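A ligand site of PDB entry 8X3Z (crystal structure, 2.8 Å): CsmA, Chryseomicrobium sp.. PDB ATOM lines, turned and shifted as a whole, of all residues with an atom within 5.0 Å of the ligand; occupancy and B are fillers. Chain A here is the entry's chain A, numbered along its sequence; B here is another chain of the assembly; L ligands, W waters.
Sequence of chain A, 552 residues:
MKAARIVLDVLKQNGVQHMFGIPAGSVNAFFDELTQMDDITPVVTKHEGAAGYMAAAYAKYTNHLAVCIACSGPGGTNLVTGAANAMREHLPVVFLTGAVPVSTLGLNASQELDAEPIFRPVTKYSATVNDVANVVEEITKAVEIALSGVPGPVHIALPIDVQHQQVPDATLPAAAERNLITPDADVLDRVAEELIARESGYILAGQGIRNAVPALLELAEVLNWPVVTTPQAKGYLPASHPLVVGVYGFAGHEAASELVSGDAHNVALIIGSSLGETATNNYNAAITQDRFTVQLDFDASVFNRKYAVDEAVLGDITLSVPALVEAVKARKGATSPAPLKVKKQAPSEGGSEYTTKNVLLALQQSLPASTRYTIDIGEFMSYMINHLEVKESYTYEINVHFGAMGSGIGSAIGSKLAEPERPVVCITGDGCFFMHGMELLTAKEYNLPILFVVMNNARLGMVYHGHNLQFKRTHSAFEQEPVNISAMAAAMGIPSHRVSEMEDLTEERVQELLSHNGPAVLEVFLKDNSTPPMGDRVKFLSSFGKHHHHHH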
ATOM      1  N   ARG A  88      -1.525 -17.855 -17.430  1.00  0.00           N
ATOM      2  CA  ARG A  88      -1.146 -18.594 -16.242  1.00  0.00           C
ATOM      3  C   ARG A  88      -0.988 -17.682 -15.032  1.00  0.00           C
ATOM      4  O   ARG A  88      -1.268 -18.097 -13.904  1.00  0.00           O
ATOM      5  CB  ARG A  88       0.148 -19.389 -16.524  1.00  0.00           C
ATOM      6  CG  ARG A  88       0.836 -19.960 -15.317  1.00  0.00           C
ATOM      7  CD  ARG A  88       0.014 -21.096 -14.714  1.00  0.00           C
ATOM      8  NE  ARG A  88       0.666 -21.634 -13.529  1.00  0.00           N
ATOM      9  CZ  ARG A  88       0.561 -21.092 -12.328  1.00  0.00           C
ATOM     10  NH1 ARG A  88      -0.164 -19.980 -12.164  1.00  0.00           N
ATOM     11  NH2 ARG A  88       1.195 -21.637 -11.281  1.00  0.00           N
ATOM     12  N   GLU A  89      -0.558 -16.439 -15.251  1.00  0.00           N
ATOM     13  CA  GLU A  89      -0.310 -15.501 -14.159  1.00  0.00           C
ATOM     14  C   GLU A  89      -1.544 -14.704 -13.756  1.00  0.00           C
ATOM     15  O   GLU A  89      -1.477 -13.953 -12.793  1.00  0.00           O
ATOM     16  CB  GLU A  89       0.850 -14.549 -14.546  1.00  0.00           C
ATOM     17  CG  GLU A  89       2.187 -15.279 -14.678  1.00  0.00           C
ATOM     18  CD  GLU A  89       2.573 -16.077 -13.428  1.00  0.00           C
ATOM     19  OE1 GLU A  89       2.736 -17.306 -13.480  1.00  0.00           O
ATOM     20  OE2 GLU A  89       2.727 -15.421 -12.378  1.00  0.00           O
ATOM     21  N   HIS A  90      -2.663 -14.883 -14.449  1.00  0.00           N
ATOM     22  CA  HIS A  90      -3.894 -14.104 -14.213  1.00  0.00           C
ATOM     23  C   HIS A  90      -3.655 -12.603 -14.356  1.00  0.00           C
ATOM     24  O   HIS A  90      -4.181 -11.790 -13.594  1.00  0.00           O
ATOM     25  CB  HIS A  90      -4.485 -14.430 -12.840  1.00  0.00           C
ATOM     26  CG  HIS A  90      -4.856 -15.862 -12.640  1.00  0.00           C
ATOM     27  ND1 HIS A  90      -5.587 -16.577 -13.557  1.00  0.00           N
ATOM     28  CD2 HIS A  90      -4.626 -16.704 -11.608  1.00  0.00           C
ATOM     29  CE1 HIS A  90      -5.787 -17.803 -13.111  1.00  0.00           C
ATOM     30  NE2 HIS A  90      -5.204 -17.904 -11.931  1.00  0.00           N
ATOM     31  N   VAL A 150     -11.509 -13.293 -12.144  1.00  0.00           N
ATOM     32  CA  VAL A 150     -10.113 -13.694 -12.159  1.00  0.00           C
ATOM     33  C   VAL A 150      -9.485 -13.065 -13.400  1.00  0.00           C
ATOM     34  O   VAL A 150      -9.737 -13.551 -14.515  1.00  0.00           O
ATOM     35  CB  VAL A 150      -9.944 -15.227 -12.197  1.00  0.00           C
ATOM     36  CG1 VAL A 150      -8.446 -15.608 -12.266  1.00  0.00           C
ATOM     37  CG2 VAL A 150     -10.602 -15.873 -10.982  1.00  0.00           C
ATOM     38  N   GLY A 206       1.285 -17.755  -1.145  1.00  0.00           N
ATOM     39  CA  GLY A 206       1.655 -17.707  -2.547  1.00  0.00           C
ATOM     40  C   GLY A 206       1.529 -16.288  -3.106  1.00  0.00           C
ATOM     41  O   GLY A 206       1.254 -15.318  -2.382  1.00  0.00           O
ATOM     42  N   GLN A 207       1.719 -16.165  -4.411  1.00  0.00           N
ATOM     43  CA  GLN A 207       1.810 -14.813  -4.941  1.00  0.00           C
ATOM     44  C   GLN A 207       0.468 -14.079  -4.977  1.00  0.00           C
ATOM     45  O   GLN A 207       0.443 -12.862  -5.170  1.00  0.00           O
ATOM     46  CB  GLN A 207       2.477 -14.845  -6.311  1.00  0.00           C
ATOM     47  CG  GLN A 207       1.607 -15.385  -7.415  1.00  0.00           C
ATOM     48  CD  GLN A 207       2.207 -15.112  -8.778  1.00  0.00           C
ATOM     49  OE1 GLN A 207       3.092 -14.259  -8.942  1.00  0.00           O
ATOM     50  NE2 GLN A 207       1.712 -15.837  -9.769  1.00  0.00           N
ATOM     51  N   GLY A 208      -0.636 -14.766  -4.705  1.00  0.00           N
ATOM     52  CA  GLY A 208      -1.908 -14.066  -4.622  1.00  0.00           C
ATOM     53  C   GLY A 208      -2.037 -13.086  -3.470  1.00  0.00           C
ATOM     54  O   GLY A 208      -3.061 -12.390  -3.382  1.00  0.00           O
ATOM     55  N   ARG A 210      -0.005 -10.649  -3.153  1.00  0.00           N
ATOM     56  CA  ARG A 210       0.886  -9.562  -3.545  1.00  0.00           C
ATOM     57  C   ARG A 210       0.272  -8.164  -3.364  1.00  0.00           C
ATOM     58  O   ARG A 210       1.011  -7.215  -3.088  1.00  0.00           O
ATOM     59  CB  ARG A 210       1.372  -9.840  -4.960  1.00  0.00           C
ATOM     60  CG  ARG A 210       0.602  -9.214  -6.029  1.00  0.00           C
ATOM     61  CD  ARG A 210       1.277  -9.498  -7.324  1.00  0.00           C
ATOM     62  NE  ARG A 210       0.432  -9.077  -8.424  1.00  0.00           N
ATOM     63  CZ  ARG A 210      -0.395  -9.896  -9.068  1.00  0.00           C
ATOM     64  NH1 ARG A 210      -0.490 -11.189  -8.716  1.00  0.00           N
ATOM     65  NH2 ARG A 210      -1.132  -9.400 -10.066  1.00  0.00           N
ATOM     66  N   THR A 230       5.774 -19.300  -1.055  1.00  0.00           N
ATOM     67  CA  THR A 230       6.145 -20.085  -2.221  1.00  0.00           C
ATOM     68  C   THR A 230       7.398 -19.456  -2.838  1.00  0.00           C
ATOM     69  O   THR A 230       7.679 -18.271  -2.617  1.00  0.00           O
ATOM     70  CB  THR A 230       5.034 -20.090  -3.258  1.00  0.00           C
ATOM     71  OG1 THR A 230       4.930 -18.780  -3.843  1.00  0.00           O
ATOM     72  CG2 THR A 230       3.683 -20.493  -2.657  1.00  0.00           C
ATOM     73  N   GLN A 232       7.733 -18.453  -5.850  1.00  0.00           N
ATOM     74  CA  GLN A 232       7.243 -17.314  -6.621  1.00  0.00           C
ATOM     75  C   GLN A 232       6.959 -16.093  -5.758  1.00  0.00           C
ATOM     76  O   GLN A 232       7.037 -14.963  -6.233  1.00  0.00           O
ATOM     77  CB  GLN A 232       5.972 -17.740  -7.382  1.00  0.00           C
ATOM     78  CG  GLN A 232       5.308 -16.651  -8.214  1.00  0.00           C
ATOM     79  CD  GLN A 232       5.632 -16.735  -9.712  1.00  0.00           C
ATOM     80  OE1 GLN A 232       6.507 -17.491 -10.148  1.00  0.00           O
ATOM     81  NE2 GLN A 232       4.886 -15.961 -10.507  1.00  0.00           N
ATOM     82  N   ALA A 233       6.596 -16.288  -4.489  1.00  0.00           N
ATOM     83  CA  ALA A 233       6.266 -15.154  -3.633  1.00  0.00           C
ATOM     84  C   ALA A 233       7.407 -14.746  -2.716  1.00  0.00           C
ATOM     85  O   ALA A 233       7.160 -13.989  -1.774  1.00  0.00           O
ATOM     86  CB  ALA A 233       5.005 -15.442  -2.816  1.00  0.00           C
ATOM     87  N   GLY A 272      -3.587 -17.810  -1.345  1.00  0.00           N
ATOM     88  CA  GLY A 272      -3.131 -17.285  -2.614  1.00  0.00           C
ATOM     89  C   GLY A 272      -2.023 -18.097  -3.250  1.00  0.00           C
ATOM     90  O   GLY A 272      -1.026 -17.518  -3.697  1.00  0.00           O
ATOM     91  N   SER A 273      -2.149 -19.424  -3.244  1.00  0.00           N
ATOM     92  CA  SER A 273      -1.259 -20.349  -3.952  1.00  0.00           C
ATOM     93  C   SER A 273      -2.095 -21.417  -4.642  1.00  0.00           C
ATOM     94  O   SER A 273      -3.028 -21.962  -4.048  1.00  0.00           O
ATOM     95  CB  SER A 273      -0.296 -21.037  -3.010  1.00  0.00           C
ATOM     96  OG  SER A 273       0.500 -21.945  -3.745  1.00  0.00           O
ATOM     97  N   SER A 274      -1.788 -21.696  -5.902  1.00  0.00           N
ATOM     98  CA  SER A 274      -2.524 -22.743  -6.588  1.00  0.00           C
ATOM     99  C   SER A 274      -2.015 -24.117  -6.212  1.00  0.00           C
ATOM    100  O   SER A 274      -2.589 -25.122  -6.644  1.00  0.00           O
ATOM    101  CB  SER A 274      -2.498 -22.581  -8.115  1.00  0.00           C
ATOM    102  OG  SER A 274      -1.181 -22.565  -8.665  1.00  0.00           O
ATOM    103  N   LEU A 275      -0.958 -24.188  -5.413  1.00  0.00           N
ATOM    104  CA  LEU A 275      -0.475 -25.467  -4.932  1.00  0.00           C
ATOM    105  C   LEU A 275      -0.040 -26.326  -6.118  1.00  0.00           C
ATOM    106  O   LEU A 275      -0.441 -27.472  -6.276  1.00  0.00           O
ATOM    107  CB  LEU A 275      -1.541 -26.174  -4.091  1.00  0.00           C
ATOM    108  CG  LEU A 275      -1.925 -25.476  -2.778  1.00  0.00           C
ATOM    109  CD1 LEU A 275      -3.055 -26.256  -2.025  1.00  0.00           C
ATOM    110  CD2 LEU A 275      -0.714 -25.225  -1.876  1.00  0.00           C
ATOM    111  N   THR A 278       5.912 -26.112  -8.010  1.00  0.00           N
ATOM    112  CA  THR A 278       7.017 -25.447  -7.337  1.00  0.00           C
ATOM    113  C   THR A 278       6.626 -24.927  -5.960  1.00  0.00           C
ATOM    114  O   THR A 278       7.513 -24.748  -5.114  1.00  0.00           O
ATOM    115  CB  THR A 278       7.605 -24.298  -8.196  1.00  0.00           C
ATOM    116  OG1 THR A 278       6.603 -23.310  -8.454  1.00  0.00           O
ATOM    117  CG2 THR A 278       8.138 -24.836  -9.518  1.00  0.00           C
ATOM    118  N   ALA A 279       5.337 -24.795  -5.689  1.00  0.00           N
ATOM    119  CA  ALA A 279       4.896 -24.400  -4.356  1.00  0.00           C
ATOM    120  C   ALA A 279       4.853 -25.571  -3.381  1.00  0.00           C
ATOM    121  O   ALA A 279       4.853 -25.343  -2.167  1.00  0.00           O
ATOM    122  CB  ALA A 279       3.523 -23.751  -4.423  1.00  0.00           C
ATOM    123  N   LEU A 296      -7.528 -19.748   0.740  1.00  0.00           N
ATOM    124  CA  LEU A 296      -8.117 -18.501   0.261  1.00  0.00           C
ATOM    125  C   LEU A 296      -7.671 -18.283  -1.183  1.00  0.00           C
ATOM    126  O   LEU A 296      -6.474 -18.199  -1.452  1.00  0.00           O
ATOM    127  CB  LEU A 296      -7.668 -17.309   1.124  1.00  0.00           C
ATOM    128  CG  LEU A 296      -8.472 -16.972   2.391  1.00  0.00           C
ATOM    129  CD1 LEU A 296      -8.467 -18.149   3.384  1.00  0.00           C
ATOM    130  CD2 LEU A 296      -7.902 -15.728   3.040  1.00  0.00           C
ATOM    131  N   ASP A 297      -8.630 -18.212  -2.105  1.00  0.00           N
ATOM    132  CA  ASP A 297      -8.291 -18.042  -3.513  1.00  0.00           C
ATOM    133  C   ASP A 297      -9.500 -17.443  -4.236  1.00  0.00           C
ATOM    134  O   ASP A 297     -10.633 -17.704  -3.853  1.00  0.00           O
ATOM    135  CB  ASP A 297      -7.905 -19.391  -4.114  1.00  0.00           C
ATOM    136  CG  ASP A 297      -6.958 -19.284  -5.296  1.00  0.00           C
ATOM    137  OD1 ASP A 297      -7.413 -18.890  -6.404  1.00  0.00           O
ATOM    138  OD2 ASP A 297      -5.758 -19.617  -5.117  1.00  0.00           O
ATOM    139  N   PHE A 298      -9.248 -16.658  -5.301  1.00  0.00           N
ATOM    140  CA  PHE A 298     -10.367 -16.133  -6.079  1.00  0.00           C
ATOM    141  C   PHE A 298     -10.717 -16.978  -7.293  1.00  0.00           C
ATOM    142  O   PHE A 298     -11.700 -16.664  -7.980  1.00  0.00           O
ATOM    143  CB  PHE A 298     -10.176 -14.648  -6.509  1.00  0.00           C
ATOM    144  CG  PHE A 298      -9.003 -14.350  -7.467  1.00  0.00           C
ATOM    145  CD1 PHE A 298      -8.834 -15.055  -8.670  1.00  0.00           C
ATOM    146  CD2 PHE A 298      -8.220 -13.228  -7.226  1.00  0.00           C
ATOM    147  CE1 PHE A 298      -7.807 -14.734  -9.555  1.00  0.00           C
ATOM    148  CE2 PHE A 298      -7.184 -12.848  -8.065  1.00  0.00           C
ATOM    149  CZ  PHE A 298      -6.944 -13.620  -9.223  1.00  0.00           C
ATOM    150  N   ASP A 299      -9.988 -18.055  -7.562  1.00  0.00           N
ATOM    151  CA  ASP A 299     -10.270 -18.914  -8.705  1.00  0.00           C
ATOM    152  C   ASP A 299     -10.870 -20.214  -8.188  1.00  0.00           C
ATOM    153  O   ASP A 299     -10.173 -21.032  -7.605  1.00  0.00           O
ATOM    154  CB  ASP A 299      -8.991 -19.182  -9.493  1.00  0.00           C
ATOM    155  CG  ASP A 299      -9.171 -20.235 -10.593  1.00  0.00           C
ATOM    156  OD1 ASP A 299     -10.279 -20.783 -10.750  1.00  0.00           O
ATOM    157  OD2 ASP A 299      -8.203 -20.533 -11.321  1.00  0.00           O
ATOM    158  N   VAL A 302      -9.360 -23.873  -8.350  1.00  0.00           N
ATOM    159  CA  VAL A 302      -8.136 -24.372  -7.736  1.00  0.00           C
ATOM    160  C   VAL A 302      -8.393 -25.276  -6.539  1.00  0.00           C
ATOM    161  O   VAL A 302      -7.532 -26.109  -6.244  1.00  0.00           O
ATOM    162  CB  VAL A 302      -7.168 -23.302  -7.228  1.00  0.00           C
ATOM    163  CG1 VAL A 302      -6.790 -22.372  -8.270  1.00  0.00           C
ATOM    164  CG2 VAL A 302      -7.739 -22.601  -6.021  1.00  0.00           C
ATOM    165  N   GLY A 315     -12.846 -15.790  -2.915  1.00  0.00           N
ATOM    166  CA  GLY A 315     -12.836 -14.351  -2.808  1.00  0.00           C
ATOM    167  C   GLY A 315     -11.452 -13.777  -3.030  1.00  0.00           C
ATOM    168  O   GLY A 315     -10.436 -14.414  -2.825  1.00  0.00           O
ATOM    169  N   ASP A 316     -11.442 -12.514  -3.450  1.00  0.00           N
ATOM    170  CA  ASP A 316     -10.213 -11.790  -3.667  1.00  0.00           C
ATOM    171  C   ASP A 316      -9.500 -11.513  -2.339  1.00  0.00           C
ATOM    172  O   ASP A 316     -10.106 -11.005  -1.368  1.00  0.00           O
ATOM    173  CB  ASP A 316     -10.560 -10.485  -4.393  1.00  0.00           C
ATOM    174  CG  ASP A 316      -9.356  -9.733  -4.924  1.00  0.00           C
ATOM    175  OD1 ASP A 316      -8.566  -9.211  -4.109  1.00  0.00           O
ATOM    176  OD2 ASP A 316      -9.236  -9.590  -6.151  1.00  0.00           O
ATOM    177  N   ILE A 317      -8.181 -11.768  -2.331  1.00  0.00           N
ATOM    178  CA  ILE A 317      -7.356 -11.629  -1.133  1.00  0.00           C
ATOM    179  C   ILE A 317      -7.443 -10.210  -0.583  1.00  0.00           C
ATOM    180  O   ILE A 317      -7.401 -10.010   0.639  1.00  0.00           O
ATOM    181  CB  ILE A 317      -5.877 -12.004  -1.455  1.00  0.00           C
ATOM    182  CG1 ILE A 317      -5.718 -13.449  -1.938  1.00  0.00           C
ATOM    183  CG2 ILE A 317      -4.919 -11.703  -0.292  1.00  0.00           C
ATOM    184  CD1 ILE A 317      -6.310 -14.435  -1.097  1.00  0.00           C
ATOM    185  N   THR A 318      -7.570  -9.221  -1.454  1.00  0.00           N
ATOM    186  CA  THR A 318      -7.628  -7.832  -0.989  1.00  0.00           C
ATOM    187  C   THR A 318      -8.931  -7.522  -0.275  1.00  0.00           C
ATOM    188  O   THR A 318      -8.995  -6.501   0.407  1.00  0.00           O
ATOM    189  CB  THR A 318      -7.407  -6.844  -2.169  1.00  0.00           C
ATOM    190  OG1 THR A 318      -8.415  -7.022  -3.188  1.00  0.00           O
ATOM    191  CG2 THR A 318      -6.044  -7.038  -2.799  1.00  0.00           C
ATOM    192  N   HIS A 401       6.763 -20.815 -13.053  1.00  0.00           N
ATOM    193  CA  HIS A 401       5.535 -21.385 -13.556  1.00  0.00           C
ATOM    194  C   HIS A 401       5.689 -21.714 -15.029  1.00  0.00           C
ATOM    195  O   HIS A 401       6.171 -22.748 -15.361  1.00  0.00           O
ATOM    196  CB  HIS A 401       4.396 -20.449 -13.353  1.00  0.00           C
ATOM    197  CG  HIS A 401       4.139 -20.121 -11.932  1.00  0.00           C
ATOM    198  ND1 HIS A 401       3.505 -18.987 -11.541  1.00  0.00           N
ATOM    199  CD2 HIS A 401       4.393 -20.799 -10.800  1.00  0.00           C
ATOM    200  CE1 HIS A 401       3.404 -18.962 -10.242  1.00  0.00           C
ATOM    201  NE2 HIS A 401       3.933 -20.060  -9.765  1.00  0.00           N
ATOM    202  N   ASN B 108      -1.348 -27.285 -12.493  1.00  0.00           N
ATOM    203  CA  ASN B 108      -0.332 -26.244 -12.648  1.00  0.00           C
ATOM    204  C   ASN B 108       1.089 -26.783 -12.364  1.00  0.00           C
ATOM    205  O   ASN B 108       1.823 -26.295 -11.506  1.00  0.00           O
ATOM    206  CB  ASN B 108      -0.660 -25.014 -11.781  1.00  0.00           C
ATOM    207  CG  ASN B 108      -1.858 -24.229 -12.301  1.00  0.00           C
ATOM    208  OD1 ASN B 108      -2.366 -23.319 -11.634  1.00  0.00           O
ATOM    209  ND2 ASN B 108      -2.315 -24.585 -13.508  1.00  0.00           N
HETATM  210  P1  LIG L   1       2.484 -19.718  -6.402  1.00  0.00           P
HETATM  211  O1  LIG L   1       1.529 -20.790  -5.905  1.00  0.00           O
HETATM  212  O2  LIG L   1       2.914 -18.653  -5.449  1.00  0.00           O
HETATM  213  O3  LIG L   1       3.680 -20.311  -7.110  1.00  0.00           O
HETATM  214  P2  LIG L   1       0.486 -19.400  -8.467  1.00  0.00           P
HETATM  215  O4  LIG L   1       0.309 -18.401  -9.583  1.00  0.00           O
HETATM  216  O5  LIG L   1       0.603 -20.870  -8.784  1.00  0.00           O
HETATM  217  O6  LIG L   1       1.682 -18.851  -7.505  1.00  0.00           O
HETATM  218  O7  LIG L   1      -0.723 -19.270  -7.448  1.00  0.00           O
HETATM  219  C1  LIG L   1      -1.341 -17.998  -7.284  1.00  0.00           C
HETATM  220  C2  LIG L   1      -2.818 -18.244  -6.965  1.00  0.00           C
HETATM  221  O8  LIG L   1      -3.323 -17.090  -6.237  1.00  0.00           O
HETATM  222  C3  LIG L   1      -3.837 -18.472  -8.094  1.00  0.00           C
HETATM  223  O9  LIG L   1      -4.533 -19.639  -7.641  1.00  0.00           O
HETATM  224  C4  LIG L   1      -4.733 -17.245  -8.188  1.00  0.00           C
HETATM  225  O10 LIG L   1      -6.063 -17.660  -8.463  1.00  0.00           O
HETATM  226  C5  LIG L   1      -4.577 -16.637  -6.801  1.00  0.00           C
HETATM  227  N1  LIG L   1      -4.635 -15.165  -6.717  1.00  0.00           N
HETATM  228  C6  LIG L   1      -3.900 -14.204  -7.299  1.00  0.00           C
HETATM  229  N2  LIG L   1      -4.318 -12.954  -6.909  1.00  0.00           N
HETATM  230  C7  LIG L   1      -5.315 -13.147  -6.042  1.00  0.00           C
HETATM  231  C8  LIG L   1      -6.222 -12.304  -5.273  1.00  0.00           C
HETATM  232  N3  LIG L   1      -6.094 -10.981  -5.347  1.00  0.00           N
HETATM  233  N4  LIG L   1      -7.180 -12.896  -4.521  1.00  0.00           N
HETATM  234  C9  LIG L   1      -7.332 -14.246  -4.456  1.00  0.00           C
HETATM  235  N5  LIG L   1      -6.543 -15.114  -5.145  1.00  0.00           N
HETATM  236  C10 LIG L   1      -5.551 -14.614  -5.944  1.00  0.00           C
HETATM  237  O   HOH W   1       6.123 -20.926  -6.345  1.00  0.00           O
HETATM  238  O   HOH W   2      -1.812 -17.416 -10.927  1.00  0.00           O
HETATM  239  O   HOH W   3      -1.700 -14.751  -9.714  1.00  0.00           O
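O7 of the ligand lies within hydrogen-bond range of N of Ser 274 (3.1 Å). The side-chain hydroxyl (OG) of Ser 274 lies within hydrogen-bond range of an oxygen (O5) of the ligand, at 2.5 Å. An oxygen (O2) of the ligand lies within hydrogen-bond range of the side-chain hydroxyl (OG1) of Thr 230, at 2.6 Å. An oxygen (O1) of the ligand lies within hydrogen-bond range of the side-chain hydroxyl (OG) of Ser 273 (2.7 Å). The backbone NH (N) of Ile 317 sits at hydrogen-bond distance from a nitrogen (N4) of the ligand (2.7 Å). The guanidinium group (NH2) of Arg 88 is in salt-bridge range of an oxygen (O5) of the ligand (2.7 Å). A ring nitrogen (NE2) of His 401 is in hydrogen-bond range of an oxygen (O3) of the ligand. An oxygen (O10) of the ligand is in hydrogen-bond range of the side-chain carboxylate (OD1) of Asp 297 (2.8 Å). N of Phe 298 is in hydrogen-bond range of N5 of the ligand. N of Gln 207 is in hydrogen-bond range of O2 of the ligand. NE2 of Gln 207 sits at hydrogen-bond distance from O4 of the ligand (2.9 Å). N3 of the ligand is in hydrogen-bond range of OD1 of Asp 316, 3.3 Å away.
OD1 of Asn 108 of chain B sits at hydrogen-bond distance from OG of Ser 274 (3.3 Å). The side-chain hydroxyl (OG1) of Thr 230 sits close to the backbone NH (N) of Gln 232 (3.5 Å). N of Ala 233 lies within hydrogen-bond range of OG1 of Thr 230, at 3.1 Å. The side-chain hydroxyl of Ser 273 sits close to the backbone NH of Leu 275 (3.2 Å). A ring nitrogen (ND1) of His 401 lies within hydrogen-bond range of the side-chain carboxylate (OE1) of Glu 89, 2.7 Å away. The backbone NH of Gln 207 is in hydrogen-bond range of the backbone carbonyl oxygen of Gly 272, at 3.1 Å. OE1 of Gln 207 sits at hydrogen-bond distance from NE2 of Gln 232, 2.9 Å away. OE2 of Glu 89 sits at hydrogen-bond distance from NE2 of Gln 232, at 2.9 Å.
The backbone carbonyl oxygen (O) of Gly 272 lies close to an oxygen (O8) of the ligand, 3.5 Å away. CD2 of His 90 touches C4 of the ligand, 3.5 Å away. Gly 206 touches the ligand. Gly 208 touches the ligand (CA to C6, 3.3 Å). CB of Gln 232 touches O3 of the ligand, at 3.5 Å. Ala 279 touches the ligand. Asp 299 touches the ligand. Val 302 touches the ligand. Gly 315 touches the ligand (O to C9, 3.5 Å).
Water W1 lies within hydrogen-bond range of an oxygen (O3) of the ligand (2.6 Å), the backbone NH (N) of Gln 232 (3.0 Å) and the side-chain hydroxyl (OG1) of Thr 278 (3.2 Å). Water W2 bridges O4 of the ligand (2.7 Å) and O of Arg 88 (3.1 Å).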
